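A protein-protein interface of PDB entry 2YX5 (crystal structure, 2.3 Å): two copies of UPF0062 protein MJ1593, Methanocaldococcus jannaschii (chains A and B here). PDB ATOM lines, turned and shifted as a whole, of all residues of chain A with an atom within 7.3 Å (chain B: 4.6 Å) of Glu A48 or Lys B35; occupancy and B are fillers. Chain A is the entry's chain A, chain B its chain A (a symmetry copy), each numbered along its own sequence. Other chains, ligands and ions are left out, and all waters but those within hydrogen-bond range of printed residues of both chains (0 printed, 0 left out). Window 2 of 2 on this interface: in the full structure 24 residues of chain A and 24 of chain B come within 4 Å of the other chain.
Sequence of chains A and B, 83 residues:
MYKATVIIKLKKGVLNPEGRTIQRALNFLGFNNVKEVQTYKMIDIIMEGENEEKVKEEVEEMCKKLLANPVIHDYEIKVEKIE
N of Lys B35 is in hydrogen-bond range of O of Ile A46 (2.8 Å).
N of Ile A46 is in hydrogen-bond range of O of Glu B36 (2.7 Å).
The backbone NH (N) of Glu A48 is in hydrogen-bond range of the backbone carbonyl oxygen (O) of Asn B33 (3.1 Å).
The side-chain carboxylate (OE1) of Glu A58 is in hydrogen-bond range of the side-chain amide nitrogen (ND2) of Asn B33, at 2.9 Å.
The backbone NH (N) of Tyr A2 sits at hydrogen-bond distance from the backbone carbonyl oxygen (O) of Met A47 (2.8 Å).
O of Lys B35 lies within hydrogen-bond range of NE2 of Gln B23.
Val B34 touches Ile A45.
Ile A45 touches Glu B36.
Ile A46 touches Val B34 (O to C, 3.8 Å).
CA of Met A47 touches O of Asn B33, at 3.3 Å.
Met A47 touches Val B34 (CB to CA, 3.8 Å).
Glu A48 touches Lys B35.
Printed residues of chain B within 4 Å of Ile A46: Val B34, Lys B35 and Glu B36.
Of the printed residues of chain B, Met A47 touches Asn B33 (3.3 Å) and Val B34 (3.8 Å).
Glu A48 touches just these residues of chain B: Asn B33 and Lys B35.
Of the printed residues of chain B, Glu A58 touches Asn B33 (2.9 Å).
Gln B23 touches none of the printed residues of chain A.
Lys B35 touches two residues of chain A.
Of the printed residues of chain A, Glu B36 touches Ile A45 and Ile A46.
The nearest printed residue of chain B that does not touch Glu A48 is Val B34 (5.0 Å).
The nearest residue of chain A that does not touch Lys B35 is Met A47 (4.1 Å).
Printed residues of chain B that touch a printed residue of chain A: Asn B33, Val B34, Lys B35 and Glu B36.
Along chain B the printed residues that touch a printed residue of chain A span positions 33 to 36.
Hydrophobic or aromatic side chains of chain A that line the printed part of chain B: Ile A45, Ile A46 and Met A47.
Among the printed residues, 10 pairs touch across the chains.
No position is printed for both chains.
Of the 10 pairs that touch across the chains among the printed residues, none has its exchanged pair printed and touching as well.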
ATOM      1  N   MET A   1     -18.629 -22.578   3.311  1.00  0.00           N
ATOM      2  CA  MET A   1     -19.462 -21.577   2.593  1.00  0.00           C
ATOM      3  C   MET A   1     -18.712 -20.261   2.450  1.00  0.00           C
ATOM      4  O   MET A   1     -18.155 -19.711   3.413  1.00  0.00           O
ATOM      5  CB  MET A   1     -20.783 -21.351   3.329  1.00  0.00           C
ATOM      6  CG  MET A   1     -21.923 -20.991   2.406  1.00  0.00           C
ATOM      7  SD  MET A   1     -22.066 -22.218   1.087  1.00  0.00           S
ATOM      8  CE  MET A   1     -23.213 -23.423   1.818  1.00  0.00           C
ATOM      9  N   TYR A   2     -18.694 -19.769   1.220  1.00  0.00           N
ATOM     10  CA  TYR A   2     -18.011 -18.528   0.915  1.00  0.00           C
ATOM     11  C   TYR A   2     -18.895 -17.637   0.057  1.00  0.00           C
ATOM     12  O   TYR A   2     -19.759 -18.118  -0.703  1.00  0.00           O
ATOM     13  CB  TYR A   2     -16.708 -18.801   0.151  1.00  0.00           C
ATOM     14  CG  TYR A   2     -15.825 -19.897   0.720  1.00  0.00           C
ATOM     15  CD1 TYR A   2     -14.631 -19.592   1.384  1.00  0.00           C
ATOM     16  CD2 TYR A   2     -16.165 -21.241   0.553  1.00  0.00           C
ATOM     17  CE1 TYR A   2     -13.799 -20.603   1.861  1.00  0.00           C
ATOM     18  CE2 TYR A   2     -15.346 -22.255   1.023  1.00  0.00           C
ATOM     19  CZ  TYR A   2     -14.168 -21.934   1.673  1.00  0.00           C
ATOM     20  OH  TYR A   2     -13.372 -22.960   2.124  1.00  0.00           O
ATOM     21  N   ILE A  45     -21.877 -14.198  -5.336  1.00  0.00           N
ATOM     22  CA  ILE A  45     -22.039 -15.620  -5.525  1.00  0.00           C
ATOM     23  C   ILE A  45     -21.778 -16.367  -4.227  1.00  0.00           C
ATOM     24  O   ILE A  45     -20.679 -16.306  -3.679  1.00  0.00           O
ATOM     25  CB  ILE A  45     -21.095 -16.117  -6.600  1.00  0.00           C
ATOM     26  CG1 ILE A  45     -21.346 -15.323  -7.900  1.00  0.00           C
ATOM     27  CG2 ILE A  45     -21.281 -17.629  -6.776  1.00  0.00           C
ATOM     28  CD1 ILE A  45     -20.303 -15.531  -8.993  1.00  0.00           C
ATOM     29  N   ILE A  46     -22.808 -17.039  -3.719  1.00  0.00           N
ATOM     30  CA  ILE A  46     -22.678 -17.839  -2.505  1.00  0.00           C
ATOM     31  C   ILE A  46     -22.408 -19.284  -2.930  1.00  0.00           C
ATOM     32  O   ILE A  46     -23.237 -19.939  -3.591  1.00  0.00           O
ATOM     33  CB  ILE A  46     -23.930 -17.734  -1.639  1.00  0.00           C
ATOM     34  CG1 ILE A  46     -24.070 -16.282  -1.166  1.00  0.00           C
ATOM     35  CG2 ILE A  46     -23.842 -18.708  -0.461  1.00  0.00           C
ATOM     36  CD1 ILE A  46     -25.342 -15.997  -0.435  1.00  0.00           C
ATOM     37  N   MET A  47     -21.232 -19.777  -2.531  1.00  0.00           N
ATOM     38  CA  MET A  47     -20.798 -21.108  -2.955  1.00  0.00           C
ATOM     39  C   MET A  47     -19.977 -21.929  -1.947  1.00  0.00           C
ATOM     40  O   MET A  47     -19.447 -21.402  -0.951  1.00  0.00           O
ATOM     41  CB  MET A  47     -19.973 -20.919  -4.232  1.00  0.00           C
ATOM     42  CG  MET A  47     -18.936 -19.781  -4.042  1.00  0.00           C
ATOM     43  SD  MET A  47     -17.901 -19.339  -5.475  1.00  0.00           S
ATOM     44  CE  MET A  47     -17.575 -21.000  -6.185  1.00  0.00           C
ATOM     45  N   GLU A  48     -19.856 -23.223  -2.251  1.00  0.00           N
ATOM     46  CA  GLU A  48     -19.087 -24.166  -1.443  1.00  0.00           C
ATOM     47  C   GLU A  48     -17.732 -24.429  -2.098  1.00  0.00           C
ATOM     48  O   GLU A  48     -16.677 -24.111  -1.526  1.00  0.00           O
ATOM     49  CB  GLU A  48     -19.865 -25.475  -1.285  1.00  0.00           C
ATOM     50  CG  GLU A  48     -21.207 -25.277  -0.568  1.00  0.00           C
ATOM     51  CD  GLU A  48     -21.890 -26.575  -0.162  1.00  0.00           C
ATOM     52  OE1 GLU A  48     -22.103 -27.460  -1.038  1.00  0.00           O
ATOM     53  OE2 GLU A  48     -22.222 -26.703   1.045  1.00  0.00           O
ATOM     54  N   GLU A  50     -13.311 -25.313  -0.567  1.00  0.00           N
ATOM     55  CA  GLU A  50     -11.876 -25.630  -0.202  1.00  0.00           C
ATOM     56  C   GLU A  50     -11.230 -24.525   0.649  1.00  0.00           C
ATOM     57  O   GLU A  50     -10.948 -24.731   1.841  1.00  0.00           O
ATOM     58  CB  GLU A  50     -11.010 -25.856  -1.437  1.00  0.00           C
ATOM     59  CG  GLU A  50     -10.681 -27.383  -1.643  1.00  0.00           C
ATOM     60  CD  GLU A  50      -9.408 -27.637  -2.518  1.00  0.00           C
ATOM     61  OE1 GLU A  50      -8.296 -27.179  -2.193  1.00  0.00           O
ATOM     62  OE2 GLU A  50      -9.547 -28.379  -3.579  1.00  0.00           O
ATOM     63  N   ASN A  51     -11.034 -23.355   0.025  1.00  0.00           N
ATOM     64  CA  ASN A  51     -10.478 -22.166   0.690  1.00  0.00           C
ATOM     65  C   ASN A  51     -10.668 -20.975  -0.251  1.00  0.00           C
ATOM     66  O   ASN A  51     -10.903 -21.172  -1.448  1.00  0.00           O
ATOM     67  CB  ASN A  51      -8.990 -22.330   1.002  1.00  0.00           C
ATOM     68  CG  ASN A  51      -8.154 -22.452  -0.246  1.00  0.00           C
ATOM     69  OD1 ASN A  51      -8.089 -23.516  -0.868  1.00  0.00           O
ATOM     70  ND2 ASN A  51      -7.524 -21.354  -0.636  1.00  0.00           N
ATOM     71  N   VAL A  55     -11.495 -20.600  -4.383  1.00  0.00           N
ATOM     72  CA  VAL A  55     -12.822 -20.120  -4.762  1.00  0.00           C
ATOM     73  C   VAL A  55     -12.632 -19.048  -5.832  1.00  0.00           C
ATOM     74  O   VAL A  55     -13.276 -19.083  -6.891  1.00  0.00           O
ATOM     75  CB  VAL A  55     -13.567 -19.497  -3.559  1.00  0.00           C
ATOM     76  CG1 VAL A  55     -14.977 -19.122  -3.962  1.00  0.00           C
ATOM     77  CG2 VAL A  55     -13.605 -20.470  -2.403  1.00  0.00           C
ATOM     78  N   GLU A  58     -12.094 -20.384  -9.033  1.00  0.00           N
ATOM     79  CA  GLU A  58     -13.291 -20.888  -9.656  1.00  0.00           C
ATOM     80  C   GLU A  58     -14.177 -19.793 -10.271  1.00  0.00           C
ATOM     81  O   GLU A  58     -14.623 -19.923 -11.413  1.00  0.00           O
ATOM     82  CB  GLU A  58     -14.078 -21.721  -8.648  1.00  0.00           C
ATOM     83  CG  GLU A  58     -14.957 -22.785  -9.298  1.00  0.00           C
ATOM     84  CD  GLU A  58     -15.848 -23.501  -8.302  1.00  0.00           C
ATOM     85  OE1 GLU A  58     -15.358 -23.889  -7.212  1.00  0.00           O
ATOM     86  OE2 GLU A  58     -17.046 -23.687  -8.617  1.00  0.00           O
ATOM     87  N   GLN B  23     -27.498 -18.195 -11.514  1.00  0.00           N
ATOM     88  CA  GLN B  23     -27.276 -19.417 -10.764  1.00  0.00           C
ATOM     89  C   GLN B  23     -27.417 -20.641 -11.664  1.00  0.00           C
ATOM     90  O   GLN B  23     -26.482 -21.439 -11.818  1.00  0.00           O
ATOM     91  CB  GLN B  23     -28.281 -19.524  -9.631  1.00  0.00           C
ATOM     92  CG  GLN B  23     -27.981 -20.625  -8.639  1.00  0.00           C
ATOM     93  CD  GLN B  23     -29.190 -20.938  -7.809  1.00  0.00           C
ATOM     94  OE1 GLN B  23     -30.150 -21.505  -8.307  1.00  0.00           O
ATOM     95  NE2 GLN B  23     -29.166 -20.551  -6.543  1.00  0.00           N
ATOM     96  N   ASN B  32     -21.353 -26.620  -9.902  1.00  0.00           N
ATOM     97  CA  ASN B  32     -22.400 -27.035  -8.968  1.00  0.00           C
ATOM     98  C   ASN B  32     -22.151 -26.570  -7.535  1.00  0.00           C
ATOM     99  O   ASN B  32     -23.000 -26.714  -6.653  1.00  0.00           O
ATOM    100  CB  ASN B  32     -22.589 -28.538  -9.053  1.00  0.00           C
ATOM    101  CG  ASN B  32     -23.260 -28.936 -10.347  1.00  0.00           C
ATOM    102  OD1 ASN B  32     -24.391 -28.511 -10.628  1.00  0.00           O
ATOM    103  ND2 ASN B  32     -22.570 -29.737 -11.156  1.00  0.00           N
ATOM    104  N   ASN B  33     -20.962 -26.000  -7.332  1.00  0.00           N
ATOM    105  CA  ASN B  33     -20.551 -25.409  -6.043  1.00  0.00           C
ATOM    106  C   ASN B  33     -21.410 -24.174  -5.770  1.00  0.00           C
ATOM    107  O   ASN B  33     -21.743 -23.867  -4.574  1.00  0.00           O
ATOM    108  CB  ASN B  33     -19.096 -24.934  -6.144  1.00  0.00           C
ATOM    109  CG  ASN B  33     -18.168 -25.953  -5.618  1.00  0.00           C
ATOM    110  OD1 ASN B  33     -18.508 -26.627  -4.594  1.00  0.00           O
ATOM    111  ND2 ASN B  33     -16.989 -26.119  -6.254  1.00  0.00           N
ATOM    112  N   VAL B  34     -21.734 -23.450  -6.850  1.00  0.00           N
ATOM    113  CA  VAL B  34     -22.537 -22.241  -6.731  1.00  0.00           C
ATOM    114  C   VAL B  34     -23.899 -22.616  -6.198  1.00  0.00           C
ATOM    115  O   VAL B  34     -24.653 -23.371  -6.820  1.00  0.00           O
ATOM    116  CB  VAL B  34     -22.663 -21.502  -8.080  1.00  0.00           C
ATOM    117  CG1 VAL B  34     -23.465 -20.211  -7.896  1.00  0.00           C
ATOM    118  CG2 VAL B  34     -21.267 -21.185  -8.623  1.00  0.00           C
ATOM    119  N   LYS B  35     -24.206 -22.084  -5.024  1.00  0.00           N
ATOM    120  CA  LYS B  35     -25.465 -22.391  -4.383  1.00  0.00           C
ATOM    121  C   LYS B  35     -26.516 -21.297  -4.478  1.00  0.00           C
ATOM    122  O   LYS B  35     -27.711 -21.575  -4.399  1.00  0.00           O
ATOM    123  CB  LYS B  35     -25.208 -22.758  -2.916  1.00  0.00           C
ATOM    124  CG  LYS B  35     -24.576 -24.137  -2.751  1.00  0.00           C
ATOM    125  CD  LYS B  35     -25.539 -25.229  -3.211  1.00  0.00           C
ATOM    126  CE  LYS B  35     -24.964 -26.621  -3.011  1.00  0.00           C
ATOM    127  NZ  LYS B  35     -26.026 -27.659  -3.103  1.00  0.00           N
ATOM    128  N   GLU B  36     -26.074 -20.061  -4.659  1.00  0.00           N
ATOM    129  CA  GLU B  36     -27.001 -18.952  -4.734  1.00  0.00           C
ATOM    130  C   GLU B  36     -26.338 -17.705  -5.306  1.00  0.00           C
ATOM    131  O   GLU B  36     -25.169 -17.444  -5.036  1.00  0.00           O
ATOM    132  CB  GLU B  36     -27.526 -18.671  -3.339  1.00  0.00           C
ATOM    133  CG  GLU B  36     -28.458 -17.505  -3.235  1.00  0.00           C
ATOM    134  CD  GLU B  36     -29.006 -17.382  -1.839  1.00  0.00           C
ATOM    135  OE1 GLU B  36     -29.521 -18.399  -1.326  1.00  0.00           O
ATOM    136  OE2 GLU B  36     -28.925 -16.284  -1.252  1.00  0.00           O
